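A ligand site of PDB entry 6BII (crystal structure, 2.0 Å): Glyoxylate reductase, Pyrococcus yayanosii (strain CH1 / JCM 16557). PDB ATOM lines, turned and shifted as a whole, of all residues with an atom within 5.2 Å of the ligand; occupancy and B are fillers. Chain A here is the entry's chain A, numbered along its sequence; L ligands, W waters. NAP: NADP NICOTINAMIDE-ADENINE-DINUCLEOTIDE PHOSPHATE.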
ATOM      1  N   VAL A  76      -1.690  -9.448  18.711  1.00  0.00           N
ATOM      2  CA  VAL A  76      -0.609  -8.432  18.565  1.00  0.00           C
ATOM      3  C   VAL A  76      -0.062  -8.394  17.135  1.00  0.00           C
ATOM      4  O   VAL A  76       0.308  -7.323  16.612  1.00  0.00           O
ATOM      5  CB  VAL A  76       0.521  -8.595  19.633  1.00  0.00           C
ATOM      6  CG1 VAL A  76       1.230  -9.925  19.547  1.00  0.00           C
ATOM      7  CG2 VAL A  76       1.521  -7.444  19.545  1.00  0.00           C
ATOM      8  N   GLY A  77      -0.024  -9.568  16.503  1.00  0.00           N
ATOM      9  CA  GLY A  77       0.231  -9.653  15.056  1.00  0.00           C
ATOM     10  C   GLY A  77      -0.885  -9.003  14.261  1.00  0.00           C
ATOM     11  O   GLY A  77      -2.032  -8.948  14.711  1.00  0.00           O
ATOM     12  N   ASP A  79      -0.508  -9.206  10.466  1.00  0.00           N
ATOM     13  CA  ASP A  79      -0.196  -9.617   9.097  1.00  0.00           C
ATOM     14  C   ASP A  79      -1.449 -10.052   8.319  1.00  0.00           C
ATOM     15  O   ASP A  79      -1.423 -10.136   7.115  1.00  0.00           O
ATOM     16  CB  ASP A  79       0.845 -10.737   9.082  1.00  0.00           C
ATOM     17  CG  ASP A  79       0.441 -11.932   9.926  1.00  0.00           C
ATOM     18  OD1 ASP A  79       0.604 -11.862  11.164  1.00  0.00           O
ATOM     19  OD2 ASP A  79      -0.041 -12.927   9.373  1.00  0.00           O
ATOM     20  N   LEU A 100      -0.460 -10.022  26.365  1.00  0.00           N
ATOM     21  CA  LEU A 100      -0.200 -11.416  26.040  1.00  0.00           C
ATOM     22  C   LEU A 100       1.286 -11.792  26.072  1.00  0.00           C
ATOM     23  O   LEU A 100       1.656 -12.904  25.747  1.00  0.00           O
ATOM     24  CB  LEU A 100      -0.819 -11.763  24.657  1.00  0.00           C
ATOM     25  CG  LEU A 100      -0.568 -10.788  23.506  1.00  0.00           C
ATOM     26  CD1 LEU A 100       0.905 -10.556  23.207  1.00  0.00           C
ATOM     27  CD2 LEU A 100      -1.279 -11.280  22.249  1.00  0.00           C
ATOM     28  N   THR A 101       2.143 -10.864  26.463  1.00  0.00           N
ATOM     29  CA  THR A 101       3.583 -11.057  26.378  1.00  0.00           C
ATOM     30  C   THR A 101       4.023 -12.212  27.276  1.00  0.00           C
ATOM     31  O   THR A 101       4.768 -13.074  26.843  1.00  0.00           O
ATOM     32  CB  THR A 101       4.317  -9.753  26.770  1.00  0.00           C
ATOM     33  OG1 THR A 101       4.080  -8.768  25.746  1.00  0.00           O
ATOM     34  CG2 THR A 101       5.798  -9.987  26.982  1.00  0.00           C
ATOM     35  N   THR A 104       2.901 -15.746  26.107  1.00  0.00           N
ATOM     36  CA  THR A 104       3.642 -16.209  24.932  1.00  0.00           C
ATOM     37  C   THR A 104       5.101 -16.579  25.251  1.00  0.00           C
ATOM     38  O   THR A 104       5.617 -17.588  24.772  1.00  0.00           O
ATOM     39  CB  THR A 104       3.577 -15.187  23.783  1.00  0.00           C
ATOM     40  OG1 THR A 104       2.202 -14.866  23.513  1.00  0.00           O
ATOM     41  CG2 THR A 104       4.192 -15.763  22.516  1.00  0.00           C
ATOM     42  N   VAL A 156      15.571 -13.987  18.012  1.00  0.00           N
ATOM     43  CA  VAL A 156      15.405 -13.343  16.711  1.00  0.00           C
ATOM     44  C   VAL A 156      14.135 -12.507  16.782  1.00  0.00           C
ATOM     45  O   VAL A 156      13.045 -13.045  16.801  1.00  0.00           O
ATOM     46  CB  VAL A 156      15.363 -14.343  15.553  1.00  0.00           C
ATOM     47  CG1 VAL A 156      15.199 -13.622  14.230  1.00  0.00           C
ATOM     48  CG2 VAL A 156      16.661 -15.125  15.487  1.00  0.00           C
ATOM     49  N   GLY A 157      14.311 -11.187  16.827  1.00  0.00           N
ATOM     50  CA  GLY A 157      13.232 -10.267  17.163  1.00  0.00           C
ATOM     51  C   GLY A 157      13.337  -9.933  18.657  1.00  0.00           C
ATOM     52  O   GLY A 157      13.257 -10.807  19.501  1.00  0.00           O
ATOM     53  N   PHE A 158      13.533  -8.667  18.982  1.00  0.00           N
ATOM     54  CA  PHE A 158      13.820  -8.286  20.380  1.00  0.00           C
ATOM     55  C   PHE A 158      12.935  -7.142  20.796  1.00  0.00           C
ATOM     56  O   PHE A 158      13.396  -6.107  21.291  1.00  0.00           O
ATOM     57  CB  PHE A 158      15.306  -7.974  20.563  1.00  0.00           C
ATOM     58  CG  PHE A 158      15.838  -8.302  21.948  1.00  0.00           C
ATOM     59  CD1 PHE A 158      15.671  -9.539  22.507  1.00  0.00           C
ATOM     60  CD2 PHE A 158      16.589  -7.373  22.647  1.00  0.00           C
ATOM     61  CE1 PHE A 158      16.185  -9.824  23.763  1.00  0.00           C
ATOM     62  CE2 PHE A 158      17.111  -7.662  23.892  1.00  0.00           C
ATOM     63  CZ  PHE A 158      16.928  -8.882  24.442  1.00  0.00           C
ATOM     64  N   GLY A 159      11.635  -7.348  20.586  1.00  0.00           N
ATOM     65  CA  GLY A 159      10.600  -6.461  21.048  1.00  0.00           C
ATOM     66  C   GLY A 159      10.040  -6.962  22.376  1.00  0.00           C
ATOM     67  O   GLY A 159      10.744  -7.457  23.225  1.00  0.00           O
ATOM     68  N   ARG A 160       8.747  -6.849  22.523  1.00  0.00           N
ATOM     69  CA  ARG A 160       8.079  -7.167  23.782  1.00  0.00           C
ATOM     70  C   ARG A 160       8.257  -8.651  24.145  1.00  0.00           C
ATOM     71  O   ARG A 160       8.702  -8.970  25.260  1.00  0.00           O
ATOM     72  CB  ARG A 160       6.603  -6.794  23.667  1.00  0.00           C
ATOM     73  CG  ARG A 160       6.354  -5.279  23.504  1.00  0.00           C
ATOM     74  CD  ARG A 160       4.915  -4.996  23.073  1.00  0.00           C
ATOM     75  NE  ARG A 160       4.637  -5.426  21.675  1.00  0.00           N
ATOM     76  CZ  ARG A 160       4.301  -4.614  20.668  1.00  0.00           C
ATOM     77  NH1 ARG A 160       4.160  -3.290  20.867  1.00  0.00           N
ATOM     78  NH2 ARG A 160       4.062  -5.126  19.457  1.00  0.00           N
ATOM     79  N   ILE A 161       7.991  -9.543  23.198  1.00  0.00           N
ATOM     80  CA  ILE A 161       8.036 -10.979  23.478  1.00  0.00           C
ATOM     81  C   ILE A 161       9.485 -11.478  23.538  1.00  0.00           C
ATOM     82  O   ILE A 161       9.862 -12.207  24.447  1.00  0.00           O
ATOM     83  CB  ILE A 161       7.162 -11.769  22.492  1.00  0.00           C
ATOM     84  CG1 ILE A 161       5.679 -11.416  22.752  1.00  0.00           C
ATOM     85  CG2 ILE A 161       7.391 -13.261  22.677  1.00  0.00           C
ATOM     86  CD1 ILE A 161       4.737 -11.823  21.647  1.00  0.00           C
ATOM     87  N   GLY A 162      10.307 -11.030  22.599  1.00  0.00           N
ATOM     88  CA  GLY A 162      11.714 -11.387  22.642  1.00  0.00           C
ATOM     89  C   GLY A 162      12.415 -11.011  23.932  1.00  0.00           C
ATOM     90  O   GLY A 162      13.205 -11.789  24.472  1.00  0.00           O
ATOM     91  N   THR A 179      18.880 -10.367  17.725  1.00  0.00           N
ATOM     92  CA  THR A 179      18.918  -9.534  16.544  1.00  0.00           C
ATOM     93  C   THR A 179      17.563  -8.867  16.368  1.00  0.00           C
ATOM     94  O   THR A 179      16.543  -9.344  16.860  1.00  0.00           O
ATOM     95  CB  THR A 179      19.432 -10.284  15.284  1.00  0.00           C
ATOM     96  OG1 THR A 179      19.983  -9.314  14.374  1.00  0.00           O
ATOM     97  CG2 THR A 179      18.346 -11.093  14.661  1.00  0.00           C
ATOM     98  N   ALA A 180      17.589  -7.710  15.739  1.00  0.00           N
ATOM     99  CA  ALA A 180      16.392  -6.916  15.487  1.00  0.00           C
ATOM    100  C   ALA A 180      16.757  -5.913  14.410  1.00  0.00           C
ATOM    101  O   ALA A 180      17.910  -5.819  14.027  1.00  0.00           O
ATOM    102  CB  ALA A 180      15.949  -6.202  16.748  1.00  0.00           C
ATOM    103  N   ARG A 181      15.781  -5.196  13.907  1.00  0.00           N
ATOM    104  CA  ARG A 181      16.074  -4.137  12.920  1.00  0.00           C
ATOM    105  C   ARG A 181      16.769  -2.910  13.500  1.00  0.00           C
ATOM    106  O   ARG A 181      17.345  -2.130  12.751  1.00  0.00           O
ATOM    107  CB  ARG A 181      14.789  -3.758  12.163  1.00  0.00           C
ATOM    108  CG  ARG A 181      14.301  -4.871  11.250  1.00  0.00           C
ATOM    109  CD  ARG A 181      13.011  -4.518  10.554  1.00  0.00           C
ATOM    110  NE  ARG A 181      13.070  -3.294   9.728  1.00  0.00           N
ATOM    111  CZ  ARG A 181      13.489  -3.220   8.477  1.00  0.00           C
ATOM    112  NH1 ARG A 181      13.994  -4.281   7.849  1.00  0.00           N
ATOM    113  NH2 ARG A 181      13.457  -2.046   7.846  1.00  0.00           N
ATOM    114  N   SER A 182      16.718  -2.748  14.817  1.00  0.00           N
ATOM    115  CA  SER A 182      17.415  -1.657  15.510  1.00  0.00           C
ATOM    116  C   SER A 182      18.000  -2.152  16.831  1.00  0.00           C
ATOM    117  O   SER A 182      17.495  -3.127  17.422  1.00  0.00           O
ATOM    118  CB  SER A 182      16.450  -0.519  15.776  1.00  0.00           C
ATOM    119  OG  SER A 182      15.364  -1.004  16.571  1.00  0.00           O
ATOM    120  N   LYS A 184      18.934  -2.020  20.798  1.00  0.00           N
ATOM    121  CA  LYS A 184      18.099  -1.780  21.960  1.00  0.00           C
ATOM    122  C   LYS A 184      19.022  -1.568  23.171  1.00  0.00           C
ATOM    123  O   LYS A 184      19.200  -2.462  23.990  1.00  0.00           O
ATOM    124  CB  LYS A 184      17.225  -3.006  22.182  1.00  0.00           C
ATOM    125  CG  LYS A 184      16.419  -3.478  20.989  1.00  0.00           C
ATOM    126  CD  LYS A 184      15.071  -2.791  20.963  1.00  0.00           C
ATOM    127  CE  LYS A 184      14.197  -3.310  19.861  1.00  0.00           C
ATOM    128  NZ  LYS A 184      14.380  -2.468  18.721  1.00  0.00           N
ATOM    129  N   ALA A 211      10.759 -14.568  17.436  1.00  0.00           N
ATOM    130  CA  ALA A 211       9.778 -13.653  18.021  1.00  0.00           C
ATOM    131  C   ALA A 211       9.649 -12.370  17.179  1.00  0.00           C
ATOM    132  O   ALA A 211       9.620 -11.242  17.710  1.00  0.00           O
ATOM    133  CB  ALA A 211      10.191 -13.321  19.453  1.00  0.00           C
ATOM    134  N   VAL A 212       9.571 -12.567  15.871  1.00  0.00           N
ATOM    135  CA  VAL A 212       9.407 -11.514  14.886  1.00  0.00           C
ATOM    136  C   VAL A 212       7.988 -11.533  14.326  1.00  0.00           C
ATOM    137  O   VAL A 212       7.375 -12.586  14.297  1.00  0.00           O
ATOM    138  CB  VAL A 212      10.355 -11.671  13.657  1.00  0.00           C
ATOM    139  CG1 VAL A 212      11.787 -11.338  14.029  1.00  0.00           C
ATOM    140  CG2 VAL A 212      10.258 -13.060  13.007  1.00  0.00           C
ATOM    141  N   PRO A 213       7.488 -10.389  13.871  1.00  0.00           N
ATOM    142  CA  PRO A 213       6.282 -10.414  13.049  1.00  0.00           C
ATOM    143  C   PRO A 213       6.549 -11.017  11.659  1.00  0.00           C
ATOM    144  O   PRO A 213       7.687 -11.120  11.241  1.00  0.00           O
ATOM    145  CB  PRO A 213       5.893  -8.937  12.927  1.00  0.00           C
ATOM    146  CG  PRO A 213       7.070  -8.176  13.387  1.00  0.00           C
ATOM    147  CD  PRO A 213       8.133  -9.073  13.881  1.00  0.00           C
ATOM    148  N   LEU A 214       5.476 -11.434  10.977  1.00  0.00           N
ATOM    149  CA  LEU A 214       5.550 -11.817   9.580  1.00  0.00           C
ATOM    150  C   LEU A 214       5.486 -10.579   8.710  1.00  0.00           C
ATOM    151  O   LEU A 214       4.515  -9.817   8.761  1.00  0.00           O
ATOM    152  CB  LEU A 214       4.415 -12.783   9.198  1.00  0.00           C
ATOM    153  CG  LEU A 214       4.421 -13.260   7.741  1.00  0.00           C
ATOM    154  CD1 LEU A 214       5.713 -14.016   7.433  1.00  0.00           C
ATOM    155  CD2 LEU A 214       3.208 -14.143   7.479  1.00  0.00           C
ATOM    156  N   THR A 215       6.537 -10.380   7.914  1.00  0.00           N
ATOM    157  CA  THR A 215       6.607  -9.311   6.917  1.00  0.00           C
ATOM    158  C   THR A 215       7.207  -9.892   5.643  1.00  0.00           C
ATOM    159  O   THR A 215       7.640 -11.053   5.642  1.00  0.00           O
ATOM    160  CB  THR A 215       7.539  -8.168   7.385  1.00  0.00           C
ATOM    161  OG1 THR A 215       8.891  -8.663   7.459  1.00  0.00           O
ATOM    162  CG2 THR A 215       7.114  -7.654   8.778  1.00  0.00           C
ATOM    163  N   GLU A 217       9.968  -9.260   4.613  1.00  0.00           N
ATOM    164  CA  GLU A 217      11.361  -9.518   4.940  1.00  0.00           C
ATOM    165  C   GLU A 217      11.581 -10.743   5.818  1.00  0.00           C
ATOM    166  O   GLU A 217      12.599 -11.391   5.678  1.00  0.00           O
ATOM    167  CB  GLU A 217      12.035  -8.277   5.552  1.00  0.00           C
ATOM    168  CG  GLU A 217      13.519  -8.451   5.814  1.00  0.00           C
ATOM    169  CD  GLU A 217      14.243  -7.162   6.106  1.00  0.00           C
ATOM    170  OE1 GLU A 217      14.108  -6.209   5.301  1.00  0.00           O
ATOM    171  OE2 GLU A 217      14.979  -7.109   7.114  1.00  0.00           O
ATOM    172  N   THR A 218      10.657 -11.052   6.729  1.00  0.00           N
ATOM    173  CA  THR A 218      10.849 -12.219   7.600  1.00  0.00           C
ATOM    174  C   THR A 218      10.360 -13.511   6.953  1.00  0.00           C
ATOM    175  O   THR A 218      10.658 -14.582   7.475  1.00  0.00           O
ATOM    176  CB  THR A 218      10.212 -12.048   8.988  1.00  0.00           C
ATOM    177  OG1 THR A 218       8.793 -11.871   8.869  1.00  0.00           O
ATOM    178  CG2 THR A 218      10.812 -10.840   9.693  1.00  0.00           C
ATOM    179  N   MET A 221      12.736 -16.533   6.361  1.00  0.00           N
ATOM    180  CA  MET A 221      14.095 -16.104   6.761  1.00  0.00           C
ATOM    181  C   MET A 221      14.895 -17.267   7.326  1.00  0.00           C
ATOM    182  O   MET A 221      16.122 -17.326   7.157  1.00  0.00           O
ATOM    183  CB  MET A 221      14.084 -14.902   7.752  1.00  0.00           C
ATOM    184  CG  MET A 221      13.664 -15.174   9.168  1.00  0.00           C
ATOM    185  SD  MET A 221      13.540 -13.674  10.200  1.00  0.00           S
ATOM    186  CE  MET A 221      15.236 -13.209  10.260  1.00  0.00           C
ATOM    187  N   VAL A 239       7.672 -19.315  18.064  1.00  0.00           N
ATOM    188  CA  VAL A 239       6.418 -18.762  18.592  1.00  0.00           C
ATOM    189  C   VAL A 239       6.018 -17.480  17.839  1.00  0.00           C
ATOM    190  O   VAL A 239       5.183 -16.693  18.315  1.00  0.00           O
ATOM    191  CB  VAL A 239       6.454 -18.503  20.108  1.00  0.00           C
ATOM    192  CG1 VAL A 239       6.577 -19.814  20.850  1.00  0.00           C
ATOM    193  CG2 VAL A 239       7.554 -17.527  20.525  1.00  0.00           C
ATOM    194  N   ALA A 240       6.559 -17.294  16.650  1.00  0.00           N
ATOM    195  CA  ALA A 240       6.316 -16.094  15.866  1.00  0.00           C
ATOM    196  C   ALA A 240       5.152 -16.288  14.900  1.00  0.00           C
ATOM    197  O   ALA A 240       3.994 -16.130  15.300  1.00  0.00           O
ATOM    198  CB  ALA A 240       7.600 -15.667  15.166  1.00  0.00           C
ATOM    199  N   ARG A 241       5.467 -16.611  13.640  1.00  0.00           N
ATOM    200  CA  ARG A 241       4.499 -16.985  12.639  1.00  0.00           C
ATOM    201  C   ARG A 241       5.108 -18.148  11.827  1.00  0.00           C
ATOM    202  O   ARG A 241       6.336 -18.199  11.637  1.00  0.00           O
ATOM    203  CB  ARG A 241       4.200 -15.815  11.712  1.00  0.00           C
ATOM    204  CG  ARG A 241       3.324 -14.739  12.300  1.00  0.00           C
ATOM    205  CD  ARG A 241       1.891 -15.164  12.283  1.00  0.00           C
ATOM    206  NE  ARG A 241       0.965 -14.201  12.840  1.00  0.00           N
ATOM    207  CZ  ARG A 241       0.649 -14.087  14.134  1.00  0.00           C
ATOM    208  NH1 ARG A 241       1.228 -14.839  15.035  1.00  0.00           N
ATOM    209  NH2 ARG A 241      -0.276 -13.207  14.509  1.00  0.00           N
ATOM    210  N   ASP A 265       4.954 -23.685  17.676  1.00  0.00           N
ATOM    211  CA  ASP A 265       3.591 -23.326  18.051  1.00  0.00           C
ATOM    212  C   ASP A 265       2.794 -22.836  16.861  1.00  0.00           C
ATOM    213  O   ASP A 265       1.579 -22.667  16.945  1.00  0.00           O
ATOM    214  CB  ASP A 265       3.604 -22.184  19.120  1.00  0.00           C
ATOM    215  CG  ASP A 265       2.244 -21.889  19.677  1.00  0.00           C
ATOM    216  OD1 ASP A 265       1.539 -22.851  20.155  1.00  0.00           O
ATOM    217  OD2 ASP A 265       1.806 -20.706  19.637  1.00  0.00           O
ATOM    218  N   VAL A 266       3.472 -22.556  15.742  1.00  0.00           N
ATOM    219  CA  VAL A 266       2.872 -21.870  14.592  1.00  0.00           C
ATOM    220  C   VAL A 266       3.370 -22.513  13.302  1.00  0.00           C
ATOM    221  O   VAL A 266       4.491 -23.049  13.247  1.00  0.00           O
ATOM    222  CB  VAL A 266       3.210 -20.356  14.591  1.00  0.00           C
ATOM    223  CG1 VAL A 266       2.485 -19.678  15.740  1.00  0.00           C
ATOM    224  CG2 VAL A 266       4.710 -20.118  14.651  1.00  0.00           C
ATOM    225  N   HIS A 288      -0.890 -23.454  18.139  1.00  0.00           N
ATOM    226  CA  HIS A 288      -0.981 -21.990  18.177  1.00  0.00           C
ATOM    227  C   HIS A 288      -1.639 -21.503  19.462  1.00  0.00           C
ATOM    228  O   HIS A 288      -2.652 -20.781  19.438  1.00  0.00           O
ATOM    229  CB  HIS A 288      -1.691 -21.448  16.924  1.00  0.00           C
ATOM    230  CG  HIS A 288      -1.336 -20.038  16.598  1.00  0.00           C
ATOM    231  ND1 HIS A 288      -1.299 -19.552  15.303  1.00  0.00           N
ATOM    232  CD2 HIS A 288      -0.911 -19.016  17.391  1.00  0.00           C
ATOM    233  CE1 HIS A 288      -0.929 -18.288  15.321  1.00  0.00           C
ATOM    234  NE2 HIS A 288      -0.685 -17.932  16.574  1.00  0.00           N
ATOM    235  N   ILE A 289      -1.032 -21.880  20.575  1.00  0.00           N
ATOM    236  CA  ILE A 289      -1.581 -21.590  21.909  1.00  0.00           C
ATOM    237  C   ILE A 289      -0.656 -20.659  22.724  1.00  0.00           C
ATOM    238  O   ILE A 289      -0.794 -20.552  23.943  1.00  0.00           O
ATOM    239  CB  ILE A 289      -1.859 -22.876  22.686  1.00  0.00           C
ATOM    240  CG1 ILE A 289      -0.565 -23.712  22.884  1.00  0.00           C
ATOM    241  CG2 ILE A 289      -2.951 -23.655  21.982  1.00  0.00           C
ATOM    242  CD1 ILE A 289      -0.720 -24.911  23.824  1.00  0.00           C
ATOM    243  N   GLY A 290       0.246 -19.947  22.052  1.00  0.00           N
ATOM    244  CA  GLY A 290       1.100 -18.984  22.715  1.00  0.00           C
ATOM    245  C   GLY A 290       0.416 -18.089  23.754  1.00  0.00           C
ATOM    246  O   GLY A 290       0.921 -17.965  24.884  1.00  0.00           O
ATOM    247  N   SER A 291      -0.698 -17.458  23.403  1.00  0.00           N
ATOM    248  CA  SER A 291      -1.385 -16.539  24.321  1.00  0.00           C
ATOM    249  C   SER A 291      -2.485 -17.207  25.121  1.00  0.00           C
ATOM    250  O   SER A 291      -3.331 -16.516  25.721  1.00  0.00           O
ATOM    251  CB  SER A 291      -1.924 -15.309  23.577  1.00  0.00           C
ATOM    252  OG  SER A 291      -3.008 -15.613  22.713  1.00  0.00           O
HETATM  253  PA  NAP L   1       7.330  -6.292  18.641  1.00  0.00           P
HETATM  254  O1A NAP L   1       7.369  -5.792  20.101  1.00  0.00           O
HETATM  255  O2A NAP L   1       6.968  -5.380  17.474  1.00  0.00           O
HETATM  256  O5B NAP L   1       8.693  -7.056  18.394  1.00  0.00           O
HETATM  257  C5B NAP L   1       9.087  -7.546  17.096  1.00  0.00           C
HETATM  258  C4B NAP L   1      10.600  -7.566  16.967  1.00  0.00           C
HETATM  259  O4B NAP L   1      10.937  -8.158  15.719  1.00  0.00           O
HETATM  260  C3B NAP L   1      11.229  -6.166  16.957  1.00  0.00           C
HETATM  261  O3B NAP L   1      12.418  -6.168  17.752  1.00  0.00           O
HETATM  262  C2B NAP L   1      11.577  -5.952  15.482  1.00  0.00           C
HETATM  263  O2B NAP L   1      12.665  -5.051  15.225  1.00  0.00           O
HETATM  264  C1B NAP L   1      11.939  -7.370  15.082  1.00  0.00           C
HETATM  265  N9A NAP L   1      12.056  -7.567  13.625  1.00  0.00           N
HETATM  266  C8A NAP L   1      11.175  -7.163  12.650  1.00  0.00           C
HETATM  267  N7A NAP L   1      11.597  -7.491  11.446  1.00  0.00           N
HETATM  268  C5A NAP L   1      12.809  -8.138  11.663  1.00  0.00           C
HETATM  269  C6A NAP L   1      13.748  -8.709  10.785  1.00  0.00           C
HETATM  270  N6A NAP L   1      13.519  -8.687   9.453  1.00  0.00           N
HETATM  271  N1A NAP L   1      14.847  -9.298  11.289  1.00  0.00           N
HETATM  272  C2A NAP L   1      15.045  -9.315  12.625  1.00  0.00           C
HETATM  273  N3A NAP L   1      14.208  -8.802  13.560  1.00  0.00           N
HETATM  274  C4A NAP L   1      13.095  -8.210  13.017  1.00  0.00           C
HETATM  275  O3  NAP L   1       6.272  -7.474  18.676  1.00  0.00           O
HETATM  276  PN  NAP L   1       5.915  -8.544  19.813  1.00  0.00           P
HETATM  277  O1N NAP L   1       4.824  -8.043  20.673  1.00  0.00           O
HETATM  278  O2N NAP L   1       7.218  -8.993  20.378  1.00  0.00           O
HETATM  279  O5D NAP L   1       5.284  -9.733  18.881  1.00  0.00           O
HETATM  280  C5D NAP L   1       6.090 -10.373  17.861  1.00  0.00           C
HETATM  281  C4D NAP L   1       5.280 -11.362  17.031  1.00  0.00           C
HETATM  282  O4D NAP L   1       4.983 -12.564  17.758  1.00  0.00           O
HETATM  283  C3D NAP L   1       3.916 -10.892  16.606  1.00  0.00           C
HETATM  284  O3D NAP L   1       4.014  -9.981  15.497  1.00  0.00           O
HETATM  285  C2D NAP L   1       3.144 -12.172  16.260  1.00  0.00           C
HETATM  286  O2D NAP L   1       3.315 -12.524  14.869  1.00  0.00           O
HETATM  287  C1D NAP L   1       3.820 -13.184  17.193  1.00  0.00           C
HETATM  288  N1N NAP L   1       2.948 -13.742  18.262  1.00  0.00           N
HETATM  289  C2N NAP L   1       2.694 -15.067  18.339  1.00  0.00           C
HETATM  290  C3N NAP L   1       1.883 -15.603  19.360  1.00  0.00           C
HETATM  291  C7N NAP L   1       1.560 -17.071  19.469  1.00  0.00           C
HETATM  292  O7N NAP L   1       0.473 -17.414  19.949  1.00  0.00           O
HETATM  293  N7N NAP L   1       2.490 -17.956  19.062  1.00  0.00           N
HETATM  294  C4N NAP L   1       1.321 -14.711  20.301  1.00  0.00           C
HETATM  295  C5N NAP L   1       1.605 -13.346  20.218  1.00  0.00           C
HETATM  296  C6N NAP L   1       2.431 -12.908  19.178  1.00  0.00           C
HETATM  297  P2B NAP L   1      12.569  -3.520  15.748  1.00  0.00           P
HETATM  298  O1X NAP L   1      12.497  -3.564  17.283  1.00  0.00           O
HETATM  299  O2X NAP L   1      13.851  -2.803  15.276  1.00  0.00           O
HETATM  300  O3X NAP L   1      11.297  -2.905  15.197  1.00  0.00           O
HETATM  301  O   HOH W   1      16.143 -10.132   7.751  1.00  0.00           O
HETATM  302  O   HOH W   2       2.928  -7.462  15.453  1.00  0.00           O
HETATM  303  O   HOH W   3       2.878 -11.030  12.471  1.00  0.00           O
HETATM  304  O   HOH W   4      10.209  -2.710  18.515  1.00  0.00           O
HETATM  305  O   HOH W   5      13.318  -0.613  13.738  1.00  0.00           O
HETATM  306  O   HOH W   6       8.525  -3.432  16.075  1.00  0.00           O
HETATM  307  O   HOH W   7      -2.298 -18.019  20.716  1.00  0.00           O
HETATM  308  O   HOH W   8       3.338  -8.108  23.091  1.00  0.00           O
HETATM  309  O   HOH W   9      17.267 -10.228  10.595  1.00  0.00           O
HETATM  310  O   HOH W  10       9.682  -9.628  19.986  1.00  0.00           O
HETATM  311  O   HOH W  11       6.626  -2.716  17.971  1.00  0.00           O
HETATM  312  O   HOH W  12      11.058  -0.227  15.034  1.00  0.00           O
HETATM  313  O   HOH W  13      10.658  -7.052   8.843  1.00  0.00           O
HETATM  314  O   HOH W  14       4.650  -5.474  16.131  1.00  0.00           O
HETATM  315  O   HOH W  15      10.476  -3.221  12.741  1.00  0.00           O
HETATM  316  O   HOH W  16       8.344  -3.342  20.601  1.00  0.00           O
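N of Gly 159 is in hydrogen-bond range of O3B of the ligand. N7N of the ligand sits close to O of Val 239, 3.1 Å away. An oxygen (O7N) of the ligand sits close to the backbone NH (N) of Gly 290, 3.3 Å away. The backbone NH (N) of Arg 160 sits at hydrogen-bond distance from an oxygen (O1A) of the ligand (3.0 Å). An oxygen (O1X) of the ligand is in salt-bridge range of the side-chain amino group (NZ) of Lys 184. N of Ser 182 lies within hydrogen-bond range of O2X of the ligand (2.9 Å). An oxygen (O2N) of the ligand lies within hydrogen-bond range of the backbone NH of Ile 161 (3.0 Å). OE2 of Glu 217 lies within hydrogen-bond range of N6A of the ligand, 3.2 Å away. The guanidinium group (NH1) of Arg 241 is in hydrogen-bond range of an oxygen (O2D) of the ligand. The backbone NH (N) of Arg 181 is in hydrogen-bond range of an oxygen (O2X) of the ligand (3.4 Å). An oxygen (O2X) of the ligand lies within hydrogen-bond range of the side-chain hydroxyl (OG) of Ser 182. The side-chain carboxylate (OD2) of Asp 265 lies within hydrogen-bond range of a nitrogen (N7N) of the ligand (2.9 Å). The backbone NH of Phe 158 is in hydrogen-bond range of an oxygen (O3B) of the ligand (3.0 Å). O1N of the ligand lies within salt-bridge range of NE of Arg 160 (2.8 Å).
The backbone carbonyl oxygen (O) of Asp 265 is in hydrogen-bond range of the backbone NH (N) of His 288 (2.9 Å). NE of Arg 241 lies within salt-bridge range of OD1 of Asp 79. N of Thr 215 is in hydrogen-bond range of OG1 of Thr 218 (2.9 Å). The side-chain carboxylate of Asp 265 lies within hydrogen-bond range of the backbone NH of Ile 289, 2.8 Å away. OD2 of Asp 265 lies within hydrogen-bond range of N of Gly 290 (3.0 Å). The side-chain hydroxyl (OG1) of Thr 104 lies within hydrogen-bond range of the backbone carbonyl oxygen (O) of Leu 100 (3.0 Å). NH1 of Arg 181 lies within salt-bridge range of OE2 of Glu 217. N of Gly 157 lies within hydrogen-bond range of O of Thr 179 (2.9 Å).
Residues that only touch the ligand: Val 76, His 288, Thr 104, Pro 213, Gly 157, Thr 218, Ala 180, Ala 240, Val 212, Ala 211, Ser 291, Val 266 and Gly 77. Hydrophobic or aromatic side chains that line the ligand: Val 76, Ile 161, Ala 180, Val 212, Pro 213, Val 266 and His 288. Of the 35 residues printed, 25 come within 4 Å of the ligand. The nearest printed residue that does not touch the ligand is Met 221 (4.1 Å).
Water W10 lies within hydrogen-bond range of an oxygen (O2N) of the ligand, the backbone carbonyl oxygen of Ala 211, the backbone NH of Gly 162 and the backbone NH of Gly 159. Water W14 lies within hydrogen-bond range of an oxygen (O2A) of the ligand and the guanidinium group (NH2) of Arg 160. Water W2 bridges an oxygen (O3D) of the ligand and the backbone carbonyl oxygen of Val 76. Water W8 lies within hydrogen-bond range of the side-chain hydroxyl (OG1) of Thr 101 (2.8 Å), an oxygen (O1N) of the ligand (2.8 Å) and the guanidinium group (NE) of Arg 160 (3.3 Å). Water W3 lies within hydrogen-bond range of the side-chain carboxylate of Asp 79, an oxygen (O2D) of the ligand and the backbone NH of Leu 214. Water W7 lies within hydrogen-bond range of O7N of the ligand (2.9 Å), O of His 288 (3.1 Å), N of Ser 291 (3.2 Å) and N of Gly 290 (3.5 Å).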
